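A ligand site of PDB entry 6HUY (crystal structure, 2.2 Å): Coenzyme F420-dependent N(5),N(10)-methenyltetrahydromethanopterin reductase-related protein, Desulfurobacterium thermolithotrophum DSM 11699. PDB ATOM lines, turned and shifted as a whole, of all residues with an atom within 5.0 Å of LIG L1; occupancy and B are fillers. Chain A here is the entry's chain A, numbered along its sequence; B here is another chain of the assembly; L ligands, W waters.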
ATOM      1  N   TYR A  13       6.180 -17.557   8.455  1.00  0.00           N
ATOM      2  CA  TYR A  13       5.137 -16.693   7.899  1.00  0.00           C
ATOM      3  C   TYR A  13       4.388 -15.940   8.986  1.00  0.00           C
ATOM      4  O   TYR A  13       4.068 -14.761   8.818  1.00  0.00           O
ATOM      5  CB  TYR A  13       4.140 -17.493   7.052  1.00  0.00           C
ATOM      6  CG  TYR A  13       3.041 -16.596   6.528  1.00  0.00           C
ATOM      7  CD1 TYR A  13       3.192 -15.911   5.333  1.00  0.00           C
ATOM      8  CD2 TYR A  13       1.887 -16.372   7.271  1.00  0.00           C
ATOM      9  CE1 TYR A  13       2.220 -15.066   4.868  1.00  0.00           C
ATOM     10  CE2 TYR A  13       0.902 -15.521   6.809  1.00  0.00           C
ATOM     11  CZ  TYR A  13       1.074 -14.871   5.606  1.00  0.00           C
ATOM     12  OH  TYR A  13       0.111 -14.010   5.148  1.00  0.00           O
ATOM     13  N   LYS A  17       6.447 -12.607   7.778  1.00  0.00           N
ATOM     14  CA  LYS A  17       5.608 -12.179   6.655  1.00  0.00           C
ATOM     15  C   LYS A  17       4.355 -11.469   7.158  1.00  0.00           C
ATOM     16  O   LYS A  17       4.050 -10.345   6.742  1.00  0.00           O
ATOM     17  CB  LYS A  17       5.245 -13.389   5.794  1.00  0.00           C
ATOM     18  CG  LYS A  17       6.404 -13.937   4.954  1.00  0.00           C
ATOM     19  CD  LYS A  17       6.734 -13.063   3.760  1.00  0.00           C
ATOM     20  CE  LYS A  17       7.645 -13.776   2.755  1.00  0.00           C
ATOM     21  NZ  LYS A  17       7.360 -13.389   1.335  1.00  0.00           N
ATOM     22  N   LEU A  18       3.617 -12.108   8.066  1.00  0.00           N
ATOM     23  CA  LEU A  18       2.431 -11.549   8.710  1.00  0.00           C
ATOM     24  C   LEU A  18       2.679 -11.531  10.202  1.00  0.00           C
ATOM     25  O   LEU A  18       2.899 -12.586  10.813  1.00  0.00           O
ATOM     26  CB  LEU A  18       1.185 -12.381   8.389  1.00  0.00           C
ATOM     27  CG  LEU A  18      -0.132 -11.966   9.066  1.00  0.00           C
ATOM     28  CD1 LEU A  18      -0.492 -10.550   8.749  1.00  0.00           C
ATOM     29  CD2 LEU A  18      -1.260 -12.916   8.675  1.00  0.00           C
ATOM     30  N   LEU A  24      -3.330  -9.770  14.986  1.00  0.00           N
ATOM     31  CA  LEU A  24      -4.454 -10.546  15.513  1.00  0.00           C
ATOM     32  C   LEU A  24      -4.330 -10.791  17.009  1.00  0.00           C
ATOM     33  O   LEU A  24      -5.233 -10.419  17.771  1.00  0.00           O
ATOM     34  CB  LEU A  24      -4.586 -11.874  14.740  1.00  0.00           C
ATOM     35  CG  LEU A  24      -4.998 -11.713  13.271  1.00  0.00           C
ATOM     36  CD1 LEU A  24      -4.644 -12.960  12.457  1.00  0.00           C
ATOM     37  CD2 LEU A  24      -6.490 -11.400  13.112  1.00  0.00           C
ATOM     38  N   PHE A  91      -0.132 -24.595   0.713  1.00  0.00           N
ATOM     39  CA  PHE A  91      -0.978 -24.052  -0.345  1.00  0.00           C
ATOM     40  C   PHE A  91      -0.580 -24.565  -1.726  1.00  0.00           C
ATOM     41  O   PHE A  91      -1.446 -24.884  -2.544  1.00  0.00           O
ATOM     42  CB  PHE A  91      -0.878 -22.519  -0.339  1.00  0.00           C
ATOM     43  CG  PHE A  91      -1.873 -21.834   0.556  1.00  0.00           C
ATOM     44  CD1 PHE A  91      -3.226 -21.899   0.289  1.00  0.00           C
ATOM     45  CD2 PHE A  91      -1.434 -21.058   1.626  1.00  0.00           C
ATOM     46  CE1 PHE A  91      -4.140 -21.251   1.095  1.00  0.00           C
ATOM     47  CE2 PHE A  91      -2.343 -20.408   2.448  1.00  0.00           C
ATOM     48  CZ  PHE A  91      -3.693 -20.495   2.172  1.00  0.00           C
ATOM     49  N   ARG A  92       0.719 -24.561  -2.033  1.00  0.00           N
ATOM     50  CA  ARG A  92       1.149 -24.826  -3.398  1.00  0.00           C
ATOM     51  C   ARG A  92       2.074 -26.036  -3.417  1.00  0.00           C
ATOM     52  O   ARG A  92       2.633 -26.433  -2.403  1.00  0.00           O
ATOM     53  CB  ARG A  92       1.871 -23.619  -4.002  1.00  0.00           C
ATOM     54  CG  ARG A  92       0.995 -22.387  -4.223  1.00  0.00           C
ATOM     55  CD  ARG A  92       1.760 -21.298  -4.965  1.00  0.00           C
ATOM     56  NE  ARG A  92       3.078 -21.050  -4.370  1.00  0.00           N
ATOM     57  CZ  ARG A  92       3.335 -20.188  -3.388  1.00  0.00           C
ATOM     58  NH1 ARG A  92       2.371 -19.465  -2.833  1.00  0.00           N
ATOM     59  NH2 ARG A  92       4.588 -20.071  -2.949  1.00  0.00           N
ATOM     60  N   CYS A 117      -7.913 -24.482   5.250  1.00  0.00           N
ATOM     61  CA  CYS A 117      -8.094 -23.462   4.220  1.00  0.00           C
ATOM     62  C   CYS A 117      -7.256 -23.702   2.970  1.00  0.00           C
ATOM     63  O   CYS A 117      -7.512 -23.083   1.936  1.00  0.00           O
ATOM     64  CB  CYS A 117      -7.738 -22.085   4.784  1.00  0.00           C
ATOM     65  SG  CYS A 117      -5.986 -21.716   4.663  1.00  0.00           S
ATOM     66  N   HIS A 146     -11.820 -26.612   9.267  1.00  0.00           N
ATOM     67  CA  HIS A 146     -11.370 -25.318   8.795  1.00  0.00           C
ATOM     68  C   HIS A 146     -11.475 -24.282   9.926  1.00  0.00           C
ATOM     69  O   HIS A 146     -12.591 -23.988  10.358  1.00  0.00           O
ATOM     70  CB  HIS A 146     -12.226 -24.884   7.597  1.00  0.00           C
ATOM     71  CG  HIS A 146     -11.661 -23.756   6.817  1.00  0.00           C
ATOM     72  ND1 HIS A 146     -11.080 -22.653   7.407  1.00  0.00           N
ATOM     73  CD2 HIS A 146     -11.588 -23.538   5.481  1.00  0.00           C
ATOM     74  CE1 HIS A 146     -10.670 -21.814   6.474  1.00  0.00           C
ATOM     75  NE2 HIS A 146     -10.977 -22.325   5.292  1.00  0.00           N
ATOM     76  N   ALA A 148     -11.042 -21.068   9.957  1.00  0.00           N
ATOM     77  CA  ALA A 148     -11.557 -19.764   9.541  1.00  0.00           C
ATOM     78  C   ALA A 148     -10.980 -18.672  10.429  1.00  0.00           C
ATOM     79  O   ALA A 148     -11.677 -17.762  10.888  1.00  0.00           O
ATOM     80  CB  ALA A 148     -13.088 -19.729   9.563  1.00  0.00           C
ATOM     81  N   ALA A 149      -9.681 -18.812  10.699  1.00  0.00           N
ATOM     82  CA  ALA A 149      -8.906 -18.016  11.644  1.00  0.00           C
ATOM     83  C   ALA A 149      -7.561 -18.703  11.782  1.00  0.00           C
ATOM     84  O   ALA A 149      -7.403 -19.850  11.342  1.00  0.00           O
ATOM     85  CB  ALA A 149      -9.597 -17.928  13.009  1.00  0.00           C
ATOM     86  N   ILE A 150      -6.592 -18.046  12.389  1.00  0.00           N
ATOM     87  CA  ILE A 150      -5.271 -18.632  12.618  1.00  0.00           C
ATOM     88  C   ILE A 150      -5.303 -19.313  13.988  1.00  0.00           C
ATOM     89  O   ILE A 150      -5.425 -18.606  15.006  1.00  0.00           O
ATOM     90  CB  ILE A 150      -4.171 -17.565  12.536  1.00  0.00           C
ATOM     91  CG1 ILE A 150      -4.129 -16.973  11.127  1.00  0.00           C
ATOM     92  CG2 ILE A 150      -2.831 -18.184  12.904  1.00  0.00           C
ATOM     93  CD1 ILE A 150      -3.123 -15.822  10.922  1.00  0.00           C
ATOM     94  N   GLY A 203     -14.896 -19.680   4.833  1.00  0.00           N
ATOM     95  CA  GLY A 203     -13.775 -19.768   5.742  1.00  0.00           C
ATOM     96  C   GLY A 203     -12.476 -19.171   5.239  1.00  0.00           C
ATOM     97  O   GLY A 203     -11.696 -18.626   6.035  1.00  0.00           O
ATOM     98  N   ASP A 204     -12.220 -19.267   3.938  1.00  0.00           N
ATOM     99  CA  ASP A 204     -10.949 -18.785   3.393  1.00  0.00           C
ATOM    100  C   ASP A 204     -10.844 -17.272   3.529  1.00  0.00           C
ATOM    101  O   ASP A 204     -11.757 -16.583   3.999  1.00  0.00           O
ATOM    102  CB  ASP A 204     -10.797 -19.215   1.940  1.00  0.00           C
ATOM    103  CG  ASP A 204     -10.664 -20.722   1.769  1.00  0.00           C
ATOM    104  OD1 ASP A 204     -10.805 -21.478   2.762  1.00  0.00           O
ATOM    105  OD2 ASP A 204     -10.389 -21.143   0.618  1.00  0.00           O
ATOM    106  N   MET A 205      -9.672 -16.750   3.122  1.00  0.00           N
ATOM    107  CA  MET A 205      -9.436 -15.305   3.108  1.00  0.00           C
ATOM    108  C   MET A 205     -10.462 -14.564   2.259  1.00  0.00           C
ATOM    109  O   MET A 205     -10.703 -13.374   2.511  1.00  0.00           O
ATOM    110  CB  MET A 205      -8.029 -15.028   2.585  1.00  0.00           C
ATOM    111  CG  MET A 205      -7.685 -15.705   1.258  1.00  0.00           C
ATOM    112  SD  MET A 205      -6.077 -15.156   0.625  1.00  0.00           S
ATOM    113  CE  MET A 205      -5.807 -16.358  -0.677  1.00  0.00           C
ATOM    114  N   ILE A 207     -13.459 -14.644   2.506  1.00  0.00           N
ATOM    115  CA  ILE A 207     -14.621 -14.226   3.273  1.00  0.00           C
ATOM    116  C   ILE A 207     -14.848 -12.725   3.151  1.00  0.00           C
ATOM    117  O   ILE A 207     -15.967 -12.246   3.325  1.00  0.00           O
ATOM    118  CB  ILE A 207     -14.468 -14.642   4.747  1.00  0.00           C
ATOM    119  CG1 ILE A 207     -15.702 -14.211   5.560  1.00  0.00           C
ATOM    120  CG2 ILE A 207     -13.224 -14.001   5.347  1.00  0.00           C
ATOM    121  CD1 ILE A 207     -17.028 -14.731   5.031  1.00  0.00           C
ATOM    122  N   LEU B 228      -1.440  -9.756   3.447  1.00  0.00           N
ATOM    123  CA  LEU B 228      -1.244 -11.209   3.382  1.00  0.00           C
ATOM    124  C   LEU B 228      -0.037 -11.596   2.535  1.00  0.00           C
ATOM    125  O   LEU B 228       0.607 -12.609   2.813  1.00  0.00           O
ATOM    126  CB  LEU B 228      -2.485 -11.886   2.836  1.00  0.00           C
ATOM    127  CG  LEU B 228      -3.778 -11.847   3.656  1.00  0.00           C
ATOM    128  CD1 LEU B 228      -4.850 -12.675   2.953  1.00  0.00           C
ATOM    129  CD2 LEU B 228      -3.549 -12.361   5.077  1.00  0.00           C
ATOM    130  N   LYS B 229       0.276 -10.814   1.494  1.00  0.00           N
ATOM    131  CA  LYS B 229       1.410 -11.104   0.614  1.00  0.00           C
ATOM    132  C   LYS B 229       1.213 -12.426  -0.107  1.00  0.00           C
ATOM    133  O   LYS B 229       2.159 -13.186  -0.338  1.00  0.00           O
ATOM    134  CB  LYS B 229       2.722 -11.108   1.400  1.00  0.00           C
ATOM    135  CG  LYS B 229       2.893  -9.971   2.421  1.00  0.00           C
ATOM    136  CD  LYS B 229       3.500  -8.718   1.817  1.00  0.00           C
ATOM    137  CE  LYS B 229       3.973  -7.769   2.931  1.00  0.00           C
ATOM    138  NZ  LYS B 229       4.505  -6.474   2.395  1.00  0.00           N
ATOM    139  N   THR B 230      -0.037 -12.693  -0.489  1.00  0.00           N
ATOM    140  CA  THR B 230      -0.400 -13.922  -1.188  1.00  0.00           C
ATOM    141  C   THR B 230      -0.371 -13.700  -2.706  1.00  0.00           C
ATOM    142  O   THR B 230      -0.252 -12.569  -3.194  1.00  0.00           O
ATOM    143  CB  THR B 230      -1.787 -14.396  -0.729  1.00  0.00           C
ATOM    144  OG1 THR B 230      -2.098 -15.634  -1.364  1.00  0.00           O
ATOM    145  CG2 THR B 230      -2.871 -13.384  -1.072  1.00  0.00           C
ATOM    146  N   LYS B 231      -0.486 -14.795  -3.462  1.00  0.00           N
ATOM    147  CA  LYS B 231      -0.326 -14.723  -4.903  1.00  0.00           C
ATOM    148  C   LYS B 231      -1.585 -14.173  -5.582  1.00  0.00           C
ATOM    149  O   LYS B 231      -2.716 -14.424  -5.141  1.00  0.00           O
ATOM    150  CB  LYS B 231       0.014 -16.097  -5.486  1.00  0.00           C
ATOM    151  CG  LYS B 231       1.159 -16.843  -4.797  1.00  0.00           C
ATOM    152  CD  LYS B 231       2.469 -16.038  -4.714  1.00  0.00           C
ATOM    153  CE  LYS B 231       3.207 -15.968  -6.050  1.00  0.00           C
ATOM    154  NZ  LYS B 231       4.528 -15.280  -5.941  1.00  0.00           N
ATOM    155  N   MET B 234      -4.293 -16.745  -6.477  1.00  0.00           N
ATOM    156  CA  MET B 234      -5.163 -17.147  -5.377  1.00  0.00           C
ATOM    157  C   MET B 234      -6.194 -16.066  -5.072  1.00  0.00           C
ATOM    158  O   MET B 234      -7.364 -16.360  -4.795  1.00  0.00           O
ATOM    159  CB  MET B 234      -4.307 -17.469  -4.145  1.00  0.00           C
ATOM    160  CG  MET B 234      -3.528 -18.776  -4.256  1.00  0.00           C
ATOM    161  SD  MET B 234      -2.120 -18.919  -3.132  1.00  0.00           S
ATOM    162  CE  MET B 234      -2.933 -18.867  -1.532  1.00  0.00           C
ATOM    163  N   SER B 270     -15.796 -15.886  10.830  1.00  0.00           N
ATOM    164  CA  SER B 270     -14.687 -15.986   9.888  1.00  0.00           C
ATOM    165  C   SER B 270     -14.125 -14.610   9.533  1.00  0.00           C
ATOM    166  O   SER B 270     -12.914 -14.456   9.379  1.00  0.00           O
ATOM    167  CB  SER B 270     -15.158 -16.700   8.630  1.00  0.00           C
ATOM    168  OG  SER B 270     -14.114 -16.785   7.688  1.00  0.00           O
ATOM    169  N   LEU B 271     -14.991 -13.605   9.390  1.00  0.00           N
ATOM    170  CA  LEU B 271     -14.535 -12.311   8.910  1.00  0.00           C
ATOM    171  C   LEU B 271     -13.640 -11.617   9.922  1.00  0.00           C
ATOM    172  O   LEU B 271     -12.801 -10.796   9.532  1.00  0.00           O
ATOM    173  CB  LEU B 271     -15.750 -11.447   8.576  1.00  0.00           C
ATOM    174  CG  LEU B 271     -15.493 -10.103   7.884  1.00  0.00           C
ATOM    175  CD1 LEU B 271     -14.939 -10.330   6.485  1.00  0.00           C
ATOM    176  CD2 LEU B 271     -16.758  -9.300   7.826  1.00  0.00           C
ATOM    177  N   SER B 273     -11.038 -12.489  11.447  1.00  0.00           N
ATOM    178  CA  SER B 273      -9.610 -12.686  11.218  1.00  0.00           C
ATOM    179  C   SER B 273      -9.129 -12.090   9.897  1.00  0.00           C
ATOM    180  O   SER B 273      -7.932 -12.167   9.604  1.00  0.00           O
ATOM    181  CB  SER B 273      -9.261 -14.183  11.269  1.00  0.00           C
ATOM    182  OG  SER B 273      -9.294 -14.683  12.595  1.00  0.00           O
ATOM    183  N   MET B 274     -10.022 -11.516   9.102  1.00  0.00           N
ATOM    184  CA  MET B 274      -9.620 -10.785   7.904  1.00  0.00           C
ATOM    185  C   MET B 274      -9.804  -9.281   8.038  1.00  0.00           C
ATOM    186  O   MET B 274      -9.666  -8.553   7.056  1.00  0.00           O
ATOM    187  CB  MET B 274     -10.397 -11.304   6.687  1.00  0.00           C
ATOM    188  CG  MET B 274      -9.831 -12.611   6.119  1.00  0.00           C
ATOM    189  SD  MET B 274      -8.108 -12.523   5.551  1.00  0.00           S
ATOM    190  CE  MET B 274      -8.274 -11.368   4.178  1.00  0.00           C
ATOM    191  N   LEU B 276      -7.735  -6.856   9.150  1.00  0.00           N
ATOM    192  CA  LEU B 276      -6.322  -6.757   9.484  1.00  0.00           C
ATOM    193  C   LEU B 276      -5.807  -5.318   9.491  1.00  0.00           C
ATOM    194  O   LEU B 276      -4.713  -5.079  10.019  1.00  0.00           O
ATOM    195  CB  LEU B 276      -5.480  -7.582   8.494  1.00  0.00           C
ATOM    196  CG  LEU B 276      -5.808  -9.082   8.416  1.00  0.00           C
ATOM    197  CD1 LEU B 276      -5.261  -9.704   7.138  1.00  0.00           C
ATOM    198  CD2 LEU B 276      -5.247  -9.809   9.618  1.00  0.00           C
HETATM  199  N1  LIG L   1      -9.077 -15.403   8.061  1.00  0.00           N
HETATM  200  C1  LIG L   1      -9.909 -16.330   7.539  1.00  0.00           C
HETATM  201  N2  LIG L   1      -9.471 -17.261   6.677  1.00  0.00           N
HETATM  202  C2  LIG L   1      -8.202 -17.349   6.276  1.00  0.00           C
HETATM  203  C3  LIG L   1      -4.971 -15.871   7.610  1.00  0.00           C
HETATM  204  C4  LIG L   1      -1.273 -17.021   2.560  1.00  0.00           C
HETATM  205  C5  LIG L   1      -2.611 -16.822   2.208  1.00  0.00           C
HETATM  206  C6  LIG L   1      -3.549 -16.536   3.196  1.00  0.00           C
HETATM  207  C7  LIG L   1      -3.143 -16.443   4.515  1.00  0.00           C
HETATM  208  C8  LIG L   1      -1.815 -16.658   4.860  1.00  0.00           C
HETATM  209  O1  LIG L   1      -7.839 -18.237   5.481  1.00  0.00           O
HETATM  210  C9  LIG L   1      -7.231 -16.364   6.812  1.00  0.00           C
HETATM  211  N3  LIG L   1      -5.866 -16.279   6.538  1.00  0.00           N
HETATM  212  C10 LIG L   1      -5.484 -14.485   8.002  1.00  0.00           C
HETATM  213  N4  LIG L   1      -6.919 -14.455   8.282  1.00  0.00           N
HETATM  214  C11 LIG L   1      -7.758 -15.376   7.756  1.00  0.00           C
HETATM  215  N5  LIG L   1     -11.218 -16.300   7.901  1.00  0.00           N
HETATM  216  C12 LIG L   1      -3.645 -15.735   6.858  1.00  0.00           C
HETATM  217  N6  LIG L   1      -4.066 -16.194   5.541  1.00  0.00           N
HETATM  218  C13 LIG L   1      -0.865 -16.942   3.881  1.00  0.00           C
HETATM  219  C14 LIG L   1      -0.260 -17.345   1.492  1.00  0.00           C
HETATM  220  O2  LIG L   1      -0.512 -17.098   0.325  1.00  0.00           O
HETATM  221  N7  LIG L   1       0.881 -17.943   1.836  1.00  0.00           N
HETATM  222  C15 LIG L   1       1.698 -18.513   0.781  1.00  0.00           C
HETATM  223  C16 LIG L   1       2.031 -19.950   1.067  1.00  0.00           C
HETATM  224  O3  LIG L   1       2.382 -20.685   0.108  1.00  0.00           O
HETATM  225  O4  LIG L   1       1.921 -20.353   2.245  1.00  0.00           O
HETATM  226  C17 LIG L   1       2.970 -17.695   0.562  1.00  0.00           C
HETATM  227  C18 LIG L   1       3.656 -17.394   1.894  1.00  0.00           C
HETATM  228  C19 LIG L   1       4.801 -16.410   1.736  1.00  0.00           C
HETATM  229  O5  LIG L   1       5.970 -16.850   1.810  1.00  0.00           O
HETATM  230  O6  LIG L   1       4.533 -15.184   1.557  1.00  0.00           O
HETATM  231  C20 LIG L   1      -5.306 -16.425   5.414  1.00  0.00           C
HETATM  232  O1  LG2 L   2      -2.571 -19.388   6.465  1.00  0.00           O
HETATM  233 FE1  LG2 L   2      -5.207 -20.908   7.204  1.00  0.00          FE
HETATM  234  C1  LG2 L   2      -4.741 -20.783   8.953  1.00  0.00           C
HETATM  235  O2  LG2 L   2      -4.369 -20.717   9.998  1.00  0.00           O
HETATM  236  C2  LG2 L   2      -6.892 -20.451   7.695  1.00  0.00           C
HETATM  237  O3  LG2 L   2      -7.912 -20.124   8.085  1.00  0.00           O
HETATM  238  C3  LG2 L   2      -5.581 -22.735   7.378  1.00  0.00           C
HETATM  239  O4  LG2 L   2      -6.664 -23.151   7.760  1.00  0.00           O
HETATM  240  C4  LG2 L   2      -4.494 -23.722   7.036  1.00  0.00           C
HETATM  241  C5  LG2 L   2      -3.287 -22.876   6.669  1.00  0.00           C
HETATM  242  N1  LG2 L   2      -3.396 -21.470   6.749  1.00  0.00           N
HETATM  243  C6  LG2 L   2      -1.992 -23.503   6.293  1.00  0.00           C
HETATM  244  C7  LG2 L   2      -1.845 -25.000   6.256  1.00  0.00           C
HETATM  245  C8  LG2 L   2      -0.853 -22.617   5.961  1.00  0.00           C
HETATM  246  C9  LG2 L   2      -1.044 -21.145   6.003  1.00  0.00           C
HETATM  247  C10 LG2 L   2       0.119 -20.258   5.663  1.00  0.00           C
HETATM  248  C11 LG2 L   2      -2.320 -20.601   6.519  1.00  0.00           C
HETATM  249  O5  LG2 L   2       0.349 -23.138   5.588  1.00  0.00           O
HETATM  250  P1  LG2 L   2       1.599 -23.310   6.596  1.00  0.00           P
HETATM  251  O6  LG2 L   2       1.437 -22.398   7.750  1.00  0.00           O
HETATM  252  O7  LG2 L   2       2.933 -23.004   5.756  1.00  0.00           O
HETATM  253  O8  LG2 L   2       1.569 -24.843   7.051  1.00  0.00           O
HETATM  254  C12 LG2 L   2       1.891 -25.877   6.131  1.00  0.00           C
HETATM  255  C13 LG2 L   2       2.636 -26.930   6.921  1.00  0.00           C
HETATM  256  O9  LG2 L   2       2.691 -28.156   6.196  1.00  0.00           O
HETATM  257  C14 LG2 L   2       3.954 -28.750   6.469  1.00  0.00           C
HETATM  258  C15 LG2 L   2       4.931 -27.578   6.553  1.00  0.00           C
HETATM  259  O10 LG2 L   2       6.073 -27.913   7.338  1.00  0.00           O
HETATM  260  C16 LG2 L   2       4.074 -26.504   7.212  1.00  0.00           C
HETATM  261  O11 LG2 L   2       4.289 -26.484   8.629  1.00  0.00           O
HETATM  262  N2  LG2 L   2       4.374 -29.755   5.458  1.00  0.00           N
HETATM  263  C17 LG2 L   2       4.151 -31.066   5.577  1.00  0.00           C
HETATM  264  N3  LG2 L   2       3.543 -31.840   6.498  1.00  0.00           N
HETATM  265  C18 LG2 L   2       3.466 -33.174   6.340  1.00  0.00           C
HETATM  266  N4  LG2 L   2       2.841 -33.903   7.297  1.00  0.00           N
HETATM  267  N5  LG2 L   2       3.989 -33.818   5.268  1.00  0.00           N
HETATM  268  C19 LG2 L   2       4.635 -33.176   4.280  1.00  0.00           C
HETATM  269  O12 LG2 L   2       5.096 -33.790   3.285  1.00  0.00           O
HETATM  270  C20 LG2 L   2       4.737 -31.688   4.390  1.00  0.00           C
HETATM  271  N6  LG2 L   2       5.275 -30.700   3.657  1.00  0.00           N
HETATM  272  C21 LG2 L   2       5.047 -29.528   4.318  1.00  0.00           C
HETATM  273  O   HOH W   1       1.470 -23.152   2.945  1.00  0.00           O
HETATM  274  O   HOH W   2      -7.409 -18.570   2.711  1.00  0.00           O
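Water W2 bridges an oxygen (O1) of LIG L1 (2.8 Å) and the backbone NH of Met 205 (2.9 Å). Water W1 lies within hydrogen-bond range of an oxygen (O5) of LG2 L2 (2.9 Å), an oxygen (O4) of LIG L1 (2.9 Å) and the backbone NH (N) of Phe 91 (3.1 Å).
Tyr 13 touches LIG L1. Phe 91 touches LIG L1 (CD2 to O4, 3.5 Å). CB of Cys 117 touches O1 of LIG L1, 3.9 Å away. Ile 150 touches LIG L1. Asp 204 touches LIG L1. CG2 of Ile 207 touches N5 of LIG L1, 3.98 Å away. CD2 of Leu 228 of chain B touches C12 of LIG L1 (3.8 Å). Lys 229 of chain B touches LIG L1 (O to O6, 3.6 Å). CE of Met 234 of chain B touches O2 of LIG L1, 3.5 Å away. Hydrophobic or aromatic side chains within 4 Å of LIG L1: Tyr 13, Phe 91, Ile 150, Met 205, Ile 207, Leu 228 of chain B, Met 234 of chain B and Met 274 of chain B.
A nitrogen (N5) of LIG L1 is in hydrogen-bond range of the backbone carbonyl oxygen (O) of Gly 203 (3.0 Å). The side-chain hydroxyl (OG1) of Thr 230 of chain B is in hydrogen-bond range of an oxygen (O2) of LIG L1 (2.7 Å). O of Ser 273 of chain B sits at hydrogen-bond distance from N4 of LIG L1, at 2.8 Å. The backbone carbonyl oxygen of Ser 270 of chain B is in hydrogen-bond range of a nitrogen (N5) of LIG L1, 2.9 Å away. The side-chain hydroxyl (OG) of Ser 270 of chain B sits at hydrogen-bond distance from a nitrogen (N5) of LIG L1 (2.9 Å). An oxygen (O3) of LIG L1 lies within salt-bridge range of the guanidinium group (NH1) of Arg 92. The backbone NH of Met 205 sits at hydrogen-bond distance from an oxygen (O1) of LIG L1 (3.3 Å). NZ of Lys 17 is in salt-bridge range of O6 of LIG L1 (3.4 Å). O of Ala 148 lies within hydrogen-bond range of N5 of LIG L1, at 3.4 Å. SD of Met 274 of chain B lies within hydrogen-bond range of N4 of LIG L1, at 3.6 Å. The backbone NH of Cys 117 sits at hydrogen-bond distance from an oxygen (O4) of LG2 L2 (3.1 Å). An iron atom (FE1) of LG2 L2 is bound by the side-chain sulfur (SG) of Cys 117 (2.8 Å). The backbone NH (N) of Ala 149 sits at hydrogen-bond distance from an oxygen (O3) of LG2 L2, at 3.4 Å.
The side-chain hydroxyl of Ser 270 of chain B sits at hydrogen-bond distance from the backbone carbonyl oxygen of Gly 203, at 3.5 Å. The side-chain sulfur (SD) of Met 234 of chain B lies close to the side-chain hydroxyl (OG1) of Thr 230 of chain B, 3.7 Å away. The backbone carbonyl oxygen (O) of Leu 228 of chain B is in hydrogen-bond range of the side-chain hydroxyl (OH) of Tyr 13, 2.8 Å away. O of Tyr 13 is in hydrogen-bond range of N of Leu 18 (2.8 Å). The backbone NH (N) of Ala 148 lies within hydrogen-bond range of a ring nitrogen (ND1) of His 146 (3.0 Å). NE2 of His 146 lies within hydrogen-bond range of OD1 of Asp 204, at 2.7 Å.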
